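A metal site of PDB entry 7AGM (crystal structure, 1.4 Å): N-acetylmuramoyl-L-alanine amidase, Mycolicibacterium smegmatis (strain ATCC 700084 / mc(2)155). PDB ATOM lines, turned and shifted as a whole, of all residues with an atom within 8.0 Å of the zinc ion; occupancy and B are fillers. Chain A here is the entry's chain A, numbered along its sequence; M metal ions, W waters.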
ATOM      1  N   PRO A  15      14.377 -25.631  19.223  1.00  0.00           N
ATOM      2  CA  PRO A  15      14.886 -24.307  18.849  1.00  0.00           C
ATOM      3  C   PRO A  15      16.118 -23.979  19.690  1.00  0.00           C
ATOM      4  O   PRO A  15      16.032 -23.875  20.916  1.00  0.00           O
ATOM      5  CB  PRO A  15      13.717 -23.363  19.134  1.00  0.00           C
ATOM      6  CG  PRO A  15      12.860 -24.081  20.135  1.00  0.00           C
ATOM      7  CD  PRO A  15      13.109 -25.566  19.995  1.00  0.00           C
ATOM      8  N   GLY A  16      17.255 -23.848  19.020  1.00  0.00           N
ATOM      9  CA  GLY A  16      18.514 -23.736  19.729  1.00  0.00           C
ATOM     10  C   GLY A  16      18.567 -22.539  20.665  1.00  0.00           C
ATOM     11  O   GLY A  16      17.984 -21.478  20.391  1.00  0.00           O
ATOM     12  N   HIS A  17      19.244 -22.736  21.794  1.00  0.00           N
ATOM     13  CA  HIS A  17      19.610 -21.709  22.779  1.00  0.00           C
ATOM     14  C   HIS A  17      18.421 -21.294  23.631  1.00  0.00           C
ATOM     15  O   HIS A  17      17.344 -21.876  23.510  1.00  0.00           O
ATOM     16  CB  HIS A  17      20.342 -20.539  22.110  1.00  0.00           C
ATOM     17  CG  HIS A  17      21.460 -21.000  21.225  1.00  0.00           C
ATOM     18  ND1 HIS A  17      22.691 -21.358  21.720  1.00  0.00           N
ATOM     19  CD2 HIS A  17      21.508 -21.206  19.881  1.00  0.00           C
ATOM     20  CE1 HIS A  17      23.465 -21.747  20.718  1.00  0.00           C
ATOM     21  NE2 HIS A  17      22.764 -21.674  19.601  1.00  0.00           N
ATOM     22  N   GLN A  40      24.842 -24.531  28.330  1.00  0.00           N
ATOM     23  CA  GLN A  40      24.279 -23.777  27.231  1.00  0.00           C
ATOM     24  C   GLN A  40      25.265 -22.726  26.744  1.00  0.00           C
ATOM     25  O   GLN A  40      26.248 -22.405  27.412  1.00  0.00           O
ATOM     26  CB  GLN A  40      22.934 -23.114  27.590  1.00  0.00           C
ATOM     27  CG  GLN A  40      21.720 -23.949  27.234  1.00  0.00           C
ATOM     28  CD  GLN A  40      21.615 -24.237  25.744  1.00  0.00           C
ATOM     29  OE1 GLN A  40      22.230 -23.556  24.916  1.00  0.00           O
ATOM     30  NE2 GLN A  40      20.827 -25.246  25.389  1.00  0.00           N
ATOM     31  N   GLU A  41      24.991 -22.214  25.546  1.00  0.00           N
ATOM     32  CA  GLU A  41      25.677 -21.055  24.985  1.00  0.00           C
ATOM     33  C   GLU A  41      24.603 -20.054  24.622  1.00  0.00           C
ATOM     34  O   GLU A  41      23.475 -20.420  24.302  1.00  0.00           O
ATOM     35  CB  GLU A  41      26.424 -21.418  23.698  1.00  0.00           C
ATOM     36  CG  GLU A  41      27.660 -22.228  23.904  1.00  0.00           C
ATOM     37  CD  GLU A  41      28.784 -21.426  24.528  1.00  0.00           C
ATOM     38  OE1 GLU A  41      28.822 -20.193  24.345  1.00  0.00           O
ATOM     39  OE2 GLU A  41      29.633 -22.036  25.208  1.00  0.00           O
ATOM     40  N   SER A  42      24.964 -18.767  24.658  1.00  0.00           N
ATOM     41  CA  SER A  42      23.979 -17.731  24.374  1.00  0.00           C
ATOM     42  C   SER A  42      23.461 -17.811  22.939  1.00  0.00           C
ATOM     43  O   SER A  42      22.308 -17.462  22.673  1.00  0.00           O
ATOM     44  CB  SER A  42      24.584 -16.351  24.634  1.00  0.00           C
ATOM     45  OG  SER A  42      25.769 -16.176  23.885  1.00  0.00           O
ATOM     46  N   GLY A  43      24.293 -18.264  22.016  1.00  0.00           N
ATOM     47  CA  GLY A  43      23.963 -18.179  20.605  1.00  0.00           C
ATOM     48  C   GLY A  43      24.544 -16.929  19.974  1.00  0.00           C
ATOM     49  O   GLY A  43      24.966 -15.986  20.646  1.00  0.00           O
ATOM     50  N   THR A  44      24.571 -16.924  18.645  1.00  0.00           N
ATOM     51  CA  THR A  44      25.127 -15.808  17.906  1.00  0.00           C
ATOM     52  C   THR A  44      24.040 -14.759  17.667  1.00  0.00           C
ATOM     53  O   THR A  44      22.953 -14.825  18.234  1.00  0.00           O
ATOM     54  CB  THR A  44      25.856 -16.284  16.652  1.00  0.00           C
ATOM     55  OG1 THR A  44      26.601 -15.194  16.086  1.00  0.00           O
ATOM     56  CG2 THR A  44      24.875 -16.836  15.629  1.00  0.00           C
ATOM     57  N   GLU A  52      20.201 -15.163  17.635  1.00  0.00           N
ATOM     58  CA  GLU A  52      19.910 -16.510  17.176  1.00  0.00           C
ATOM     59  C   GLU A  52      18.722 -17.123  17.919  1.00  0.00           C
ATOM     60  O   GLU A  52      17.862 -17.762  17.306  1.00  0.00           O
ATOM     61  CB  GLU A  52      21.143 -17.402  17.341  1.00  0.00           C
ATOM     62  CG  GLU A  52      20.886 -18.836  16.873  1.00  0.00           C
ATOM     63  CD  GLU A  52      22.071 -19.747  17.071  1.00  0.00           C
ATOM     64  OE1 GLU A  52      23.138 -19.254  17.515  1.00  0.00           O
ATOM     65  OE2 GLU A  52      21.941 -20.966  16.805  1.00  0.00           O
ATOM     66  N   HIS A  53      18.648 -16.919  19.243  1.00  0.00           N
ATOM     67  CA  HIS A  53      17.606 -17.591  20.002  1.00  0.00           C
ATOM     68  C   HIS A  53      16.206 -17.162  19.582  1.00  0.00           C
ATOM     69  O   HIS A  53      15.270 -17.967  19.651  1.00  0.00           O
ATOM     70  CB  HIS A  53      17.833 -17.421  21.518  1.00  0.00           C
ATOM     71  CG  HIS A  53      17.530 -16.043  22.028  1.00  0.00           C
ATOM     72  ND1 HIS A  53      16.253 -15.598  22.278  1.00  0.00           N
ATOM     73  CD2 HIS A  53      18.354 -15.036  22.393  1.00  0.00           C
ATOM     74  CE1 HIS A  53      16.298 -14.372  22.764  1.00  0.00           C
ATOM     75  NE2 HIS A  53      17.561 -14.010  22.846  1.00  0.00           N
ATOM     76  N   THR A  56      15.571 -18.902  16.029  1.00  0.00           N
ATOM     77  CA  THR A  56      15.258 -20.324  16.116  1.00  0.00           C
ATOM     78  C   THR A  56      13.871 -20.531  16.730  1.00  0.00           C
ATOM     79  O   THR A  56      13.130 -21.422  16.308  1.00  0.00           O
ATOM     80  CB  THR A  56      16.314 -21.077  16.929  1.00  0.00           C
ATOM     81  OG1 THR A  56      16.266 -20.658  18.297  1.00  0.00           O
ATOM     82  CG2 THR A  56      17.720 -20.853  16.353  1.00  0.00           C
ATOM     83  N   SER A 105      16.856 -30.106  15.470  1.00  0.00           N
ATOM     84  CA  SER A 105      17.320 -28.938  16.196  1.00  0.00           C
ATOM     85  C   SER A 105      17.579 -27.841  15.183  1.00  0.00           C
ATOM     86  O   SER A 105      18.161 -28.081  14.125  1.00  0.00           O
ATOM     87  CB  SER A 105      18.596 -29.270  16.982  1.00  0.00           C
ATOM     88  OG  SER A 105      19.077 -28.146  17.680  1.00  0.00           O
ATOM     89  N   ILE A 106      17.089 -26.631  15.473  1.00  0.00           N
ATOM     90  CA  ILE A 106      17.130 -25.525  14.524  1.00  0.00           C
ATOM     91  C   ILE A 106      18.032 -24.428  15.084  1.00  0.00           C
ATOM     92  O   ILE A 106      17.838 -23.972  16.217  1.00  0.00           O
ATOM     93  CB  ILE A 106      15.715 -25.007  14.212  1.00  0.00           C
ATOM     94  CG1 ILE A 106      14.904 -26.106  13.529  1.00  0.00           C
ATOM     95  CG2 ILE A 106      15.788 -23.776  13.323  1.00  0.00           C
ATOM     96  CD1 ILE A 106      13.474 -25.708  13.189  1.00  0.00           C
ATOM     97  N   HIS A 107      19.011 -24.011  14.274  1.00  0.00           N
ATOM     98  CA  HIS A 107      20.056 -23.089  14.689  1.00  0.00           C
ATOM     99  C   HIS A 107      20.341 -22.090  13.579  1.00  0.00           C
ATOM    100  O   HIS A 107      19.862 -22.226  12.440  1.00  0.00           O
ATOM    101  CB  HIS A 107      21.361 -23.824  15.010  1.00  0.00           C
ATOM    102  CG  HIS A 107      21.344 -24.491  16.342  1.00  0.00           C
ATOM    103  ND1 HIS A 107      22.006 -23.982  17.431  1.00  0.00           N
ATOM    104  CD2 HIS A 107      20.722 -25.618  16.766  1.00  0.00           C
ATOM    105  CE1 HIS A 107      21.799 -24.764  18.475  1.00  0.00           C
ATOM    106  NE2 HIS A 107      21.024 -25.768  18.092  1.00  0.00           N
ATOM    107  N   ALA A 108      21.150 -21.100  13.920  1.00  0.00           N
ATOM    108  CA  ALA A 108      21.768 -20.210  12.940  1.00  0.00           C
ATOM    109  C   ALA A 108      23.226 -19.983  13.339  1.00  0.00           C
ATOM    110  O   ALA A 108      23.566 -19.992  14.526  1.00  0.00           O
ATOM    111  CB  ALA A 108      21.044 -18.859  12.821  1.00  0.00           C
ATOM    112  N   ASP A 109      24.063 -19.770  12.339  1.00  0.00           N
ATOM    113  CA  ASP A 109      25.508 -19.861  12.475  1.00  0.00           C
ATOM    114  C   ASP A 109      26.153 -18.488  12.479  1.00  0.00           C
ATOM    115  O   ASP A 109      25.559 -17.473  12.098  1.00  0.00           O
ATOM    116  CB  ASP A 109      26.070 -20.667  11.308  1.00  0.00           C
ATOM    117  CG  ASP A 109      27.408 -21.281  11.607  1.00  0.00           C
ATOM    118  OD1 ASP A 109      27.786 -21.376  12.797  1.00  0.00           O
ATOM    119  OD2 ASP A 109      28.091 -21.655  10.630  1.00  0.00           O
ATOM    120  N   GLY A 110      27.407 -18.468  12.923  1.00  0.00           N
ATOM    121  CA  GLY A 110      28.270 -17.314  12.771  1.00  0.00           C
ATOM    122  C   GLY A 110      29.525 -17.687  12.007  1.00  0.00           C
ATOM    123  O   GLY A 110      30.379 -18.407  12.531  1.00  0.00           O
ATOM    124  N   LEU A 180      20.596 -31.577  12.858  1.00  0.00           N
ATOM    125  CA  LEU A 180      20.632 -30.191  13.304  1.00  0.00           C
ATOM    126  C   LEU A 180      20.781 -29.317  12.067  1.00  0.00           C
ATOM    127  O   LEU A 180      21.727 -29.499  11.289  1.00  0.00           O
ATOM    128  CB  LEU A 180      21.770 -29.976  14.303  1.00  0.00           C
ATOM    129  CG  LEU A 180      21.874 -28.592  14.965  1.00  0.00           C
ATOM    130  CD1 LEU A 180      22.697 -28.676  16.241  1.00  0.00           C
ATOM    131  CD2 LEU A 180      22.458 -27.513  14.044  1.00  0.00           C
ATOM    132  N   VAL A 181      19.844 -28.392  11.860  1.00  0.00           N
ATOM    133  CA  VAL A 181      19.852 -27.527  10.691  1.00  0.00           C
ATOM    134  C   VAL A 181      20.404 -26.174  11.106  1.00  0.00           C
ATOM    135  O   VAL A 181      19.799 -25.468  11.923  1.00  0.00           O
ATOM    136  CB  VAL A 181      18.449 -27.375  10.078  1.00  0.00           C
ATOM    137  CG1 VAL A 181      18.492 -26.401   8.892  1.00  0.00           C
ATOM    138  CG2 VAL A 181      17.867 -28.725   9.665  1.00  0.00           C
ATOM    139  N   GLU A 182      21.571 -25.807  10.561  1.00  0.00           N
ATOM    140  CA  GLU A 182      22.078 -24.440  10.623  1.00  0.00           C
ATOM    141  C   GLU A 182      21.517 -23.727   9.388  1.00  0.00           C
ATOM    142  O   GLU A 182      21.941 -24.007   8.262  1.00  0.00           O
ATOM    143  CB  GLU A 182      23.603 -24.403  10.650  1.00  0.00           C
ATOM    144  CG  GLU A 182      24.236 -24.881  11.941  1.00  0.00           C
ATOM    145  CD  GLU A 182      24.198 -23.861  13.051  1.00  0.00           C
ATOM    146  OE1 GLU A 182      23.634 -22.773  12.830  1.00  0.00           O
ATOM    147  OE2 GLU A 182      24.730 -24.138  14.154  1.00  0.00           O
ATOM    148  N   MET A 186      24.287 -15.706  10.374  1.00  0.00           N
ATOM    149  CA  MET A 186      23.738 -14.441  10.880  1.00  0.00           C
ATOM    150  C   MET A 186      24.639 -13.256  10.570  1.00  0.00           C
ATOM    151  O   MET A 186      24.171 -12.107  10.606  1.00  0.00           O
ATOM    152  CB  MET A 186      23.511 -14.517  12.390  1.00  0.00           C
ATOM    153  CG  MET A 186      22.598 -15.661  12.808  1.00  0.00           C
ATOM    154  SD  MET A 186      21.742 -15.364  14.386  1.00  0.00           S
ATOM    155  CE  MET A 186      20.256 -14.489  13.870  1.00  0.00           C
HETATM  156 ZN    ZN M   1      23.204 -22.338  17.645  1.00  0.00          ZN
HETATM  157  O   HOH W   1      25.038 -21.283  18.000  1.00  0.00           O
HETATM  158  O   HOH W   2      24.846 -23.664  18.383  1.00  0.00           O
HETATM  159  O   HOH W   3      24.367 -22.249  15.935  1.00  0.00           O
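Water W3 bridges the side-chain carboxylate (OE2) of Glu 182 (2.6 Å) and the backbone carbonyl oxygen (O) of Ala 108 (2.8 Å).
A ring nitrogen (NE2) of His 107 lies within hydrogen-bond range of the side-chain hydroxyl (OG) of Ser 105 (3.1 Å).
The backbone NH of His 107 sits at hydrogen-bond distance from the backbone carbonyl oxygen of Val 181, 2.9 Å away.
The side-chain carboxylate (OE2) of Glu 52 sits close to the backbone NH (N) of Ala 108 (3.0 Å).
The backbone NH (N) of Glu 52 is in hydrogen-bond range of the backbone carbonyl oxygen (O) of Thr 44 (2.8 Å).
The backbone carbonyl oxygen of Glu 52 lies close to the side-chain hydroxyl of Thr 56 (3.5 Å).
ND1 of His 17 sits at hydrogen-bond distance from N of Gly 43 (3.5 Å).
A ring nitrogen (ND1) of His 17 sits at hydrogen-bond distance from the backbone carbonyl oxygen of Glu 41, 2.9 Å away.
The backbone NH (N) of Ala 108 lies close to the side-chain carboxylate (OE1) of Glu 182.
Merely in contact with the zinc ion: Ala 108 (3.9 Å).
Within 4 Å of the zinc ion: His 17, Glu 52, His 107 and Ala 108.
Along chain A the residues within 4 Å of the zinc ion span positions 17 to 108.
The zinc ion is bound by ND1 of His 107 (2.0 Å), OE2 of Glu 52 (2.0 Å), water W3 (2.1 Å), NE2 of His 17 (2.1 Å), water W1 (2.1 Å) and water W2 (2.2 Å).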
